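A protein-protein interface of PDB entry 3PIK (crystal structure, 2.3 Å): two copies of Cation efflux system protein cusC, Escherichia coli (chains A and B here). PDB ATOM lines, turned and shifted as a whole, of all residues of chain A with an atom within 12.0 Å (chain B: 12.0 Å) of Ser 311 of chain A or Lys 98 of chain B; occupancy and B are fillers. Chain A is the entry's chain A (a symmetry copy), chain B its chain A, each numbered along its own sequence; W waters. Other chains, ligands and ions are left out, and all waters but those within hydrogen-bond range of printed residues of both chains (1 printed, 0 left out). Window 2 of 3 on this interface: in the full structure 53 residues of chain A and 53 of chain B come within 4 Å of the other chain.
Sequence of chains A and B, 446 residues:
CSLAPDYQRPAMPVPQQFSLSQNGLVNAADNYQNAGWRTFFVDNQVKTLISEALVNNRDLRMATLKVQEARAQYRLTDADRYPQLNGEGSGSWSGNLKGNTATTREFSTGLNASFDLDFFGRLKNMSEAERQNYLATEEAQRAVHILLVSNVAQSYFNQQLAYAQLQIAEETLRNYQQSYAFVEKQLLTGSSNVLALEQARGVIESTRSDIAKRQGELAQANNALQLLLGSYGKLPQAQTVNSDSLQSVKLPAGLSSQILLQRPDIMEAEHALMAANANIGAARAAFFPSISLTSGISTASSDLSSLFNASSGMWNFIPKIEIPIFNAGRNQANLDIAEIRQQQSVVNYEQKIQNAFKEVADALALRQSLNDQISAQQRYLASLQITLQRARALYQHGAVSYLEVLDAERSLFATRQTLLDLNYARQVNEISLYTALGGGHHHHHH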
ATOM      1  N   GLU A 106      24.565   8.683   6.574  1.00  0.00           N
ATOM      2  CA  GLU A 106      23.724   8.581   5.390  1.00  0.00           C
ATOM      3  C   GLU A 106      22.582   7.597   5.611  1.00  0.00           C
ATOM      4  O   GLU A 106      22.797   6.490   6.097  1.00  0.00           O
ATOM      5  CB  GLU A 106      24.555   8.136   4.188  1.00  0.00           C
ATOM      6  CG  GLU A 106      23.789   8.137   2.870  1.00  0.00           C
ATOM      7  CD  GLU A 106      23.609   9.538   2.311  1.00  0.00           C
ATOM      8  OE1 GLU A 106      24.268  10.468   2.821  1.00  0.00           O
ATOM      9  OE2 GLU A 106      22.811   9.711   1.369  1.00  0.00           O
ATOM     10  N   PHE A 107      21.373   8.003   5.244  1.00  0.00           N
ATOM     11  CA  PHE A 107      20.206   7.128   5.306  1.00  0.00           C
ATOM     12  C   PHE A 107      19.724   6.797   3.894  1.00  0.00           C
ATOM     13  O   PHE A 107      19.787   7.638   2.995  1.00  0.00           O
ATOM     14  CB  PHE A 107      19.066   7.807   6.072  1.00  0.00           C
ATOM     15  CG  PHE A 107      19.368   8.073   7.518  1.00  0.00           C
ATOM     16  CD1 PHE A 107      19.231   7.073   8.464  1.00  0.00           C
ATOM     17  CD2 PHE A 107      19.766   9.330   7.936  1.00  0.00           C
ATOM     18  CE1 PHE A 107      19.499   7.323   9.797  1.00  0.00           C
ATOM     19  CE2 PHE A 107      20.038   9.579   9.267  1.00  0.00           C
ATOM     20  CZ  PHE A 107      19.907   8.581  10.194  1.00  0.00           C
ATOM     21  N   SER A 108      19.227   5.586   3.695  1.00  0.00           N
ATOM     22  CA  SER A 108      18.682   5.215   2.390  1.00  0.00           C
ATOM     23  C   SER A 108      17.474   4.287   2.481  1.00  0.00           C
ATOM     24  O   SER A 108      17.266   3.614   3.486  1.00  0.00           O
ATOM     25  CB  SER A 108      19.765   4.604   1.501  1.00  0.00           C
ATOM     26  OG  SER A 108      20.708   3.894   2.278  1.00  0.00           O
ATOM     27  N   THR A 109      16.672   4.280   1.423  1.00  0.00           N
ATOM     28  CA  THR A 109      15.469   3.468   1.362  1.00  0.00           C
ATOM     29  C   THR A 109      15.268   2.998  -0.063  1.00  0.00           C
ATOM     30  O   THR A 109      15.056   3.804  -0.967  1.00  0.00           O
ATOM     31  CB  THR A 109      14.217   4.260   1.770  1.00  0.00           C
ATOM     32  OG1 THR A 109      14.573   5.277   2.709  1.00  0.00           O
ATOM     33  CG2 THR A 109      13.176   3.331   2.393  1.00  0.00           C
ATOM     34  N   ILE A 297      13.134   1.994  -7.111  1.00  0.00           N
ATOM     35  CA  ILE A 297      12.963   3.355  -6.644  1.00  0.00           C
ATOM     36  C   ILE A 297      13.764   3.444  -5.355  1.00  0.00           C
ATOM     37  O   ILE A 297      13.742   2.531  -4.533  1.00  0.00           O
ATOM     38  CB  ILE A 297      11.499   3.662  -6.337  1.00  0.00           C
ATOM     39  CG1 ILE A 297      10.657   3.530  -7.603  1.00  0.00           C
ATOM     40  CG2 ILE A 297      11.370   5.047  -5.755  1.00  0.00           C
ATOM     41  CD1 ILE A 297      11.040   4.510  -8.682  1.00  0.00           C
ATOM     42  N   SER A 298      14.464   4.550  -5.174  1.00  0.00           N
ATOM     43  CA  SER A 298      15.461   4.633  -4.130  1.00  0.00           C
ATOM     44  C   SER A 298      15.542   6.067  -3.633  1.00  0.00           C
ATOM     45  O   SER A 298      15.193   6.995  -4.356  1.00  0.00           O
ATOM     46  CB  SER A 298      16.810   4.213  -4.713  1.00  0.00           C
ATOM     47  OG  SER A 298      17.813   4.175  -3.725  1.00  0.00           O
ATOM     48  N   THR A 299      15.997   6.250  -2.398  1.00  0.00           N
ATOM     49  CA  THR A 299      16.252   7.584  -1.872  1.00  0.00           C
ATOM     50  C   THR A 299      17.466   7.541  -0.964  1.00  0.00           C
ATOM     51  O   THR A 299      17.890   6.469  -0.537  1.00  0.00           O
ATOM     52  CB  THR A 299      15.097   8.094  -1.024  1.00  0.00           C
ATOM     53  OG1 THR A 299      15.124   7.422   0.241  1.00  0.00           O
ATOM     54  CG2 THR A 299      13.763   7.839  -1.709  1.00  0.00           C
ATOM     55  N   ALA A 300      18.013   8.713  -0.662  1.00  0.00           N
ATOM     56  CA  ALA A 300      19.125   8.806   0.269  1.00  0.00           C
ATOM     57  C   ALA A 300      19.299  10.236   0.775  1.00  0.00           C
ATOM     58  O   ALA A 300      18.970  11.190   0.083  1.00  0.00           O
ATOM     59  CB  ALA A 300      20.399   8.312  -0.378  1.00  0.00           C
ATOM     60  N   SER A 301      19.805  10.375   1.994  1.00  0.00           N
ATOM     61  CA  SER A 301      20.089  11.686   2.555  1.00  0.00           C
ATOM     62  C   SER A 301      20.934  11.562   3.808  1.00  0.00           C
ATOM     63  O   SER A 301      20.931  10.518   4.469  1.00  0.00           O
ATOM     64  CB  SER A 301      18.800  12.438   2.879  1.00  0.00           C
ATOM     65  OG  SER A 301      19.104  13.690   3.475  1.00  0.00           O
ATOM     66  N   SER A 302      21.643  12.637   4.141  1.00  0.00           N
ATOM     67  CA  SER A 302      22.525  12.647   5.306  1.00  0.00           C
ATOM     68  C   SER A 302      21.734  12.862   6.591  1.00  0.00           C
ATOM     69  O   SER A 302      22.259  12.695   7.694  1.00  0.00           O
ATOM     70  CB  SER A 302      23.595  13.725   5.148  1.00  0.00           C
ATOM     71  OG  SER A 302      23.001  14.990   4.910  1.00  0.00           O
ATOM     72  N   ASP A 303      20.469  13.250   6.447  1.00  0.00           N
ATOM     73  CA  ASP A 303      19.578  13.326   7.596  1.00  0.00           C
ATOM     74  C   ASP A 303      18.193  12.763   7.260  1.00  0.00           C
ATOM     75  O   ASP A 303      17.817  12.646   6.093  1.00  0.00           O
ATOM     76  CB  ASP A 303      19.497  14.756   8.157  1.00  0.00           C
ATOM     77  CG  ASP A 303      18.799  15.719   7.223  1.00  0.00           C
ATOM     78  OD1 ASP A 303      18.380  15.304   6.126  1.00  0.00           O
ATOM     79  OD2 ASP A 303      18.672  16.906   7.591  1.00  0.00           O
ATOM     80  N   LEU A 304      17.450  12.413   8.302  1.00  0.00           N
ATOM     81  CA  LEU A 304      16.165  11.743   8.162  1.00  0.00           C
ATOM     82  C   LEU A 304      15.096  12.677   7.615  1.00  0.00           C
ATOM     83  O   LEU A 304      14.197  12.248   6.900  1.00  0.00           O
ATOM     84  CB  LEU A 304      15.725  11.199   9.527  1.00  0.00           C
ATOM     85  CG  LEU A 304      15.465   9.698   9.676  1.00  0.00           C
ATOM     86  CD1 LEU A 304      16.377   8.894   8.771  1.00  0.00           C
ATOM     87  CD2 LEU A 304      15.602   9.257  11.139  1.00  0.00           C
ATOM     88  N   SER A 305      15.188  13.957   7.950  1.00  0.00           N
ATOM     89  CA  SER A 305      14.130  14.890   7.589  1.00  0.00           C
ATOM     90  C   SER A 305      13.935  14.963   6.074  1.00  0.00           C
ATOM     91  O   SER A 305      12.826  14.764   5.577  1.00  0.00           O
ATOM     92  CB  SER A 305      14.387  16.275   8.185  1.00  0.00           C
ATOM     93  OG  SER A 305      15.515  16.890   7.604  1.00  0.00           O
ATOM     94  N   SER A 306      15.012  15.231   5.341  1.00  0.00           N
ATOM     95  CA  SER A 306      14.923  15.292   3.887  1.00  0.00           C
ATOM     96  C   SER A 306      15.104  13.929   3.230  1.00  0.00           C
ATOM     97  O   SER A 306      15.528  13.850   2.079  1.00  0.00           O
ATOM     98  CB  SER A 306      15.931  16.294   3.311  1.00  0.00           C
ATOM     99  OG  SER A 306      17.269  15.882   3.535  1.00  0.00           O
ATOM    100  N   LEU A 307      14.776  12.859   3.954  1.00  0.00           N
ATOM    101  CA  LEU A 307      14.919  11.510   3.416  1.00  0.00           C
ATOM    102  C   LEU A 307      13.928  11.269   2.288  1.00  0.00           C
ATOM    103  O   LEU A 307      14.315  11.151   1.125  1.00  0.00           O
ATOM    104  CB  LEU A 307      14.712  10.451   4.501  1.00  0.00           C
ATOM    105  CG  LEU A 307      15.543   9.164   4.370  1.00  0.00           C
ATOM    106  CD1 LEU A 307      14.867   7.988   5.069  1.00  0.00           C
ATOM    107  CD2 LEU A 307      15.829   8.824   2.920  1.00  0.00           C
ATOM    108  N   PHE A 308      12.647  11.190   2.634  1.00  0.00           N
ATOM    109  CA  PHE A 308      11.615  10.885   1.650  1.00  0.00           C
ATOM    110  C   PHE A 308      11.276  12.060   0.760  1.00  0.00           C
ATOM    111  O   PHE A 308      10.196  12.116   0.184  1.00  0.00           O
ATOM    112  CB  PHE A 308      10.360  10.369   2.336  1.00  0.00           C
ATOM    113  CG  PHE A 308      10.582   9.109   3.081  1.00  0.00           C
ATOM    114  CD1 PHE A 308      10.953   9.139   4.413  1.00  0.00           C
ATOM    115  CD2 PHE A 308      10.454   7.889   2.446  1.00  0.00           C
ATOM    116  CE1 PHE A 308      11.171   7.968   5.107  1.00  0.00           C
ATOM    117  CE2 PHE A 308      10.673   6.713   3.132  1.00  0.00           C
ATOM    118  CZ  PHE A 308      11.031   6.752   4.465  1.00  0.00           C
ATOM    119  N   ASN A 309      12.203  13.000   0.648  1.00  0.00           N
ATOM    120  CA  ASN A 309      12.044  14.093  -0.290  1.00  0.00           C
ATOM    121  C   ASN A 309      12.197  13.603  -1.720  1.00  0.00           C
ATOM    122  O   ASN A 309      13.234  13.044  -2.080  1.00  0.00           O
ATOM    123  CB  ASN A 309      13.105  15.163  -0.044  1.00  0.00           C
ATOM    124  CG  ASN A 309      12.707  16.151   1.025  1.00  0.00           C
ATOM    125  OD1 ASN A 309      13.280  17.242   1.110  1.00  0.00           O
ATOM    126  ND2 ASN A 309      11.726  15.778   1.850  1.00  0.00           N
ATOM    127  N   ALA A 310      11.170  13.803  -2.536  1.00  0.00           N
ATOM    128  CA  ALA A 310      11.390  13.775  -3.968  1.00  0.00           C
ATOM    129  C   ALA A 310      12.344  14.941  -4.153  1.00  0.00           C
ATOM    130  O   ALA A 310      11.956  16.101  -4.009  1.00  0.00           O
ATOM    131  CB  ALA A 310      10.102  14.000  -4.721  1.00  0.00           C
ATOM    132  N   SER A 311      13.594  14.608  -4.440  1.00  0.00           N
ATOM    133  CA  SER A 311      14.721  15.524  -4.361  1.00  0.00           C
ATOM    134  C   SER A 311      15.863  14.585  -4.074  1.00  0.00           C
ATOM    135  O   SER A 311      16.944  14.686  -4.653  1.00  0.00           O
ATOM    136  CB  SER A 311      14.586  16.497  -3.179  1.00  0.00           C
ATOM    137  OG  SER A 311      13.907  17.695  -3.519  1.00  0.00           O
ATOM    138  N   SER A 312      15.586  13.661  -3.159  1.00  0.00           N
ATOM    139  CA  SER A 312      16.539  12.642  -2.744  1.00  0.00           C
ATOM    140  C   SER A 312      16.283  11.326  -3.467  1.00  0.00           C
ATOM    141  O   SER A 312      17.051  10.374  -3.324  1.00  0.00           O
ATOM    142  CB  SER A 312      16.443  12.415  -1.233  1.00  0.00           C
ATOM    143  OG  SER A 312      16.740  13.600  -0.525  1.00  0.00           O
ATOM    144  N   GLY A 313      15.200  11.280  -4.238  1.00  0.00           N
ATOM    145  CA  GLY A 313      14.771  10.053  -4.886  1.00  0.00           C
ATOM    146  C   GLY A 313      15.487   9.736  -6.187  1.00  0.00           C
ATOM    147  O   GLY A 313      16.017  10.627  -6.861  1.00  0.00           O
ATOM    148  N   MET A 314      15.503   8.454  -6.537  1.00  0.00           N
ATOM    149  CA  MET A 314      16.072   7.993  -7.796  1.00  0.00           C
ATOM    150  C   MET A 314      15.333   6.763  -8.282  1.00  0.00           C
ATOM    151  O   MET A 314      15.054   5.852  -7.510  1.00  0.00           O
ATOM    152  CB  MET A 314      17.558   7.668  -7.641  1.00  0.00           C
ATOM    153  CG  MET A 314      18.468   8.886  -7.749  1.00  0.00           C
ATOM    154  SD  MET A 314      20.129   8.453  -8.296  1.00  0.00           S
ATOM    155  CE  MET A 314      20.889  10.071  -8.400  1.00  0.00           C
ATOM    156  N   TRP A 315      14.989   6.750  -9.561  1.00  0.00           N
ATOM    157  CA  TRP A 315      14.444   5.554 -10.168  1.00  0.00           C
ATOM    158  C   TRP A 315      15.619   4.866 -10.827  1.00  0.00           C
ATOM    159  O   TRP A 315      16.688   5.462 -10.973  1.00  0.00           O
ATOM    160  CB  TRP A 315      13.382   5.894 -11.207  1.00  0.00           C
ATOM    161  CG  TRP A 315      13.959   6.538 -12.428  1.00  0.00           C
ATOM    162  CD1 TRP A 315      14.046   7.876 -12.686  1.00  0.00           C
ATOM    163  CD2 TRP A 315      14.541   5.873 -13.559  1.00  0.00           C
ATOM    164  NE1 TRP A 315      14.643   8.084 -13.905  1.00  0.00           N
ATOM    165  CE2 TRP A 315      14.957   6.875 -14.461  1.00  0.00           C
ATOM    166  CE3 TRP A 315      14.747   4.532 -13.895  1.00  0.00           C
ATOM    167  CZ2 TRP A 315      15.566   6.574 -15.683  1.00  0.00           C
ATOM    168  CZ3 TRP A 315      15.356   4.235 -15.104  1.00  0.00           C
ATOM    169  CH2 TRP A 315      15.756   5.251 -15.984  1.00  0.00           C
ATOM    170  N   ASN A 316      15.420   3.621 -11.242  1.00  0.00           N
ATOM    171  CA  ASN A 316      16.528   2.798 -11.697  1.00  0.00           C
ATOM    172  C   ASN A 316      16.050   1.593 -12.508  1.00  0.00           C
ATOM    173  O   ASN A 316      14.975   1.059 -12.250  1.00  0.00           O
ATOM    174  CB  ASN A 316      17.334   2.367 -10.478  1.00  0.00           C
ATOM    175  CG  ASN A 316      18.367   1.334 -10.805  1.00  0.00           C
ATOM    176  OD1 ASN A 316      18.190   0.154 -10.511  1.00  0.00           O
ATOM    177  ND2 ASN A 316      19.461   1.766 -11.427  1.00  0.00           N
ATOM    178  N   SER B  94      19.291   5.136 -15.074  1.00  0.00           N
ATOM    179  CA  SER B  94      18.836   5.680 -13.802  1.00  0.00           C
ATOM    180  C   SER B  94      18.739   7.185 -13.907  1.00  0.00           C
ATOM    181  O   SER B  94      19.399   7.806 -14.740  1.00  0.00           O
ATOM    182  CB  SER B  94      19.787   5.309 -12.664  1.00  0.00           C
ATOM    183  OG  SER B  94      21.058   5.901 -12.843  1.00  0.00           O
ATOM    184  N   GLY B  95      17.911   7.771 -13.057  1.00  0.00           N
ATOM    185  CA  GLY B  95      17.757   9.208 -13.058  1.00  0.00           C
ATOM    186  C   GLY B  95      17.091   9.704 -11.798  1.00  0.00           C
ATOM    187  O   GLY B  95      16.583   8.919 -10.991  1.00  0.00           O
ATOM    188  N   ASN B  96      17.098  11.021 -11.634  1.00  0.00           N
ATOM    189  CA  ASN B  96      16.461  11.643 -10.495  1.00  0.00           C
ATOM    190  C   ASN B  96      14.961  11.670 -10.643  1.00  0.00           C
ATOM    191  O   ASN B  96      14.398  11.177 -11.618  1.00  0.00           O
ATOM    192  CB  ASN B  96      16.972  13.065 -10.291  1.00  0.00           C
ATOM    193  CG  ASN B  96      18.403  13.103  -9.823  1.00  0.00           C
ATOM    194  OD1 ASN B  96      18.843  12.231  -9.077  1.00  0.00           O
ATOM    195  ND2 ASN B  96      19.144  14.118 -10.264  1.00  0.00           N
ATOM    196  N   LEU B  97      14.330  12.285  -9.659  1.00  0.00           N
ATOM    197  CA  LEU B  97      12.893  12.311  -9.548  1.00  0.00           C
ATOM    198  C   LEU B  97      12.450  13.766  -9.544  1.00  0.00           C
ATOM    199  O   LEU B  97      11.258  14.066  -9.597  1.00  0.00           O
ATOM    200  CB  LEU B  97      12.514  11.653  -8.234  1.00  0.00           C
ATOM    201  CG  LEU B  97      11.486  10.535  -8.262  1.00  0.00           C
ATOM    202  CD1 LEU B  97      12.041   9.309  -7.548  1.00  0.00           C
ATOM    203  CD2 LEU B  97      10.208  11.037  -7.610  1.00  0.00           C
ATOM    204  N   LYS B  98      13.433  14.659  -9.478  1.00  0.00           N
ATOM    205  CA  LYS B  98      13.209  16.100  -9.455  1.00  0.00           C
ATOM    206  C   LYS B  98      14.554  16.811  -9.338  1.00  0.00           C
ATOM    207  O   LYS B  98      15.376  16.456  -8.491  1.00  0.00           O
ATOM    208  CB  LYS B  98      12.322  16.494  -8.272  1.00  0.00           C
ATOM    209  CG  LYS B  98      11.747  17.902  -8.379  1.00  0.00           C
ATOM    210  CD  LYS B  98      11.296  18.452  -7.029  1.00  0.00           C
ATOM    211  CE  LYS B  98      12.453  19.097  -6.273  1.00  0.00           C
ATOM    212  NZ  LYS B  98      12.020  19.668  -4.963  1.00  0.00           N
ATOM    213  N   GLY B  99      14.776  17.812 -10.186  1.00  0.00           N
ATOM    214  CA  GLY B  99      16.014  18.576 -10.168  1.00  0.00           C
ATOM    215  C   GLY B  99      17.008  18.098 -11.210  1.00  0.00           C
ATOM    216  O   GLY B  99      18.102  17.645 -10.871  1.00  0.00           O
ATOM    217  N   ASN B 100      16.623  18.227 -12.477  1.00  0.00           N
ATOM    218  CA  ASN B 100      17.346  17.651 -13.616  1.00  0.00           C
ATOM    219  C   ASN B 100      16.911  16.218 -13.869  1.00  0.00           C
ATOM    220  O   ASN B 100      17.443  15.275 -13.283  1.00  0.00           O
ATOM    221  CB  ASN B 100      18.868  17.720 -13.460  1.00  0.00           C
ATOM    222  CG  ASN B 100      19.598  16.985 -14.578  1.00  0.00           C
ATOM    223  OD1 ASN B 100      20.037  15.848 -14.410  1.00  0.00           O
ATOM    224  ND2 ASN B 100      19.716  17.632 -15.731  1.00  0.00           N
ATOM    225  N   THR B 101      15.931  16.070 -14.748  1.00  0.00           N
ATOM    226  CA  THR B 101      15.376  14.765 -15.047  1.00  0.00           C
ATOM    227  C   THR B 101      16.050  14.172 -16.287  1.00  0.00           C
ATOM    228  O   THR B 101      15.403  13.508 -17.101  1.00  0.00           O
ATOM    229  CB  THR B 101      13.844  14.848 -15.225  1.00  0.00           C
ATOM    230  OG1 THR B 101      13.302  15.759 -14.259  1.00  0.00           O
ATOM    231  CG2 THR B 101      13.200  13.482 -15.038  1.00  0.00           C
ATOM    232  N   ALA B 102      17.353  14.420 -16.429  1.00  0.00           N
ATOM    233  CA  ALA B 102      18.152  13.765 -17.468  1.00  0.00           C
ATOM    234  C   ALA B 102      18.602  12.367 -17.018  1.00  0.00           C
ATOM    235  O   ALA B 102      19.128  12.189 -15.915  1.00  0.00           O
ATOM    236  CB  ALA B 102      19.357  14.621 -17.852  1.00  0.00           C
ATOM    237  N   THR B 103      18.388  11.376 -17.875  1.00  0.00           N
ATOM    238  CA  THR B 103      18.739   9.998 -17.554  1.00  0.00           C
ATOM    239  C   THR B 103      20.239   9.734 -17.700  1.00  0.00           C
ATOM    240  O   THR B 103      20.853  10.113 -18.702  1.00  0.00           O
ATOM    241  CB  THR B 103      17.941   9.009 -18.428  1.00  0.00           C
ATOM    242  OG1 THR B 103      16.556   9.081 -18.072  1.00  0.00           O
ATOM    243  CG2 THR B 103      18.429   7.576 -18.227  1.00  0.00           C
ATOM    244  N   THR B 104      20.824   9.111 -16.679  1.00  0.00           N
ATOM    245  CA  THR B 104      22.190   8.596 -16.753  1.00  0.00           C
ATOM    246  C   THR B 104      22.163   7.165 -17.288  1.00  0.00           C
ATOM    247  O   THR B 104      21.256   6.387 -16.988  1.00  0.00           O
ATOM    248  CB  THR B 104      22.892   8.603 -15.376  1.00  0.00           C
ATOM    249  OG1 THR B 104      23.073   9.955 -14.929  1.00  0.00           O
ATOM    250  CG2 THR B 104      24.252   7.909 -15.460  1.00  0.00           C
HETATM  251  O   HOH W   1      10.969  18.240  -2.267  1.00  0.00           O
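No residue of chain B comes within 4 Å of Asn 309 of chain A. Of chain B, only Lys 98 comes within 4 Å of Ala 310 of chain A. Of chain B, only Lys 98 (3.1 Å) comes within 4 Å of Ser 311 of chain A. Of chain B, only Asn 96 (3.8 Å) and Leu 97 (3.7 Å) come within 4 Å of Gly 313 of chain A. Of the printed residues of chain B, Trp 315 of chain A touches Ser 94, Gly 95, Asn 96 and Thr 103. Of the printed residues of chain A, Ser 94 of chain B touches Trp 315 (3.5 Å) and Asn 316 (3.8 Å). Asn 96 of chain B touches three residues of chain A. Of chain A, only Ala 310 (3.7 Å) and Ser 311 (3.1 Å) come within 4 Å of Lys 98 of chain B. No residue of chain A comes within 4 Å of Gly 99 of chain B.
The backbone NH (N) of Met 314 of chain A sits at hydrogen-bond distance from the backbone carbonyl oxygen (O) of Ser 298 of chain A, 2.6 Å away. N of Thr 104 of chain B lies within hydrogen-bond range of O of Ser 94 of chain B (2.7 Å).
Hydrophobic or aromatic side chains of chain B that line the printed part of chain A: Leu 97. Among the printed residues, 12 pairs touch across the chains. Among the printed residues, no Asp or Glu carboxylate lies within 4 Å of a Lys or Arg side-chain nitrogen of the other chain.
No position is printed for both chains. Of the 12 pairs that touch across the chains among the printed residues, none has its exchanged pair printed and touching as well.
The backbone carbonyl oxygen of Gly 95 of chain B sits at hydrogen-bond distance from the backbone NH of Trp 315 of chain A, 3.0 Å away. NZ of Lys 98 of chain B lies within hydrogen-bond range of OG of Ser 311 of chain A (3.1 Å).
Among the printed residues, merely in contact across the chains: Ala 310 of chain A with Lys 98 of chain B (3.7 Å), Gly 313 of chain A with Asn 96 of chain B (3.8 Å), Gly 313 of chain A with Leu 97 of chain B (3.7 Å), Met 314 of chain A with Gly 95 of chain B (3.4 Å), Met 314 of chain A with Asn 96 of chain B (3.1 Å), Met 314 of chain A with Leu 97 of chain B (3.7 Å), Trp 315 of chain A with Ser 94 of chain B (3.5 Å), Trp 315 of chain A with Asn 96 of chain B (3.5 Å), Trp 315 of chain A with Thr 103 of chain B (3.6 Å) and Asn 316 of chain A with Ser 94 of chain B (3.8 Å).
Water W1 lies within hydrogen-bond range of O of Ala 310 of chain A (2.9 Å), NZ of Lys 98 of chain B (3.2 Å) and OG of Ser 311 of chain A (3.2 Å).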
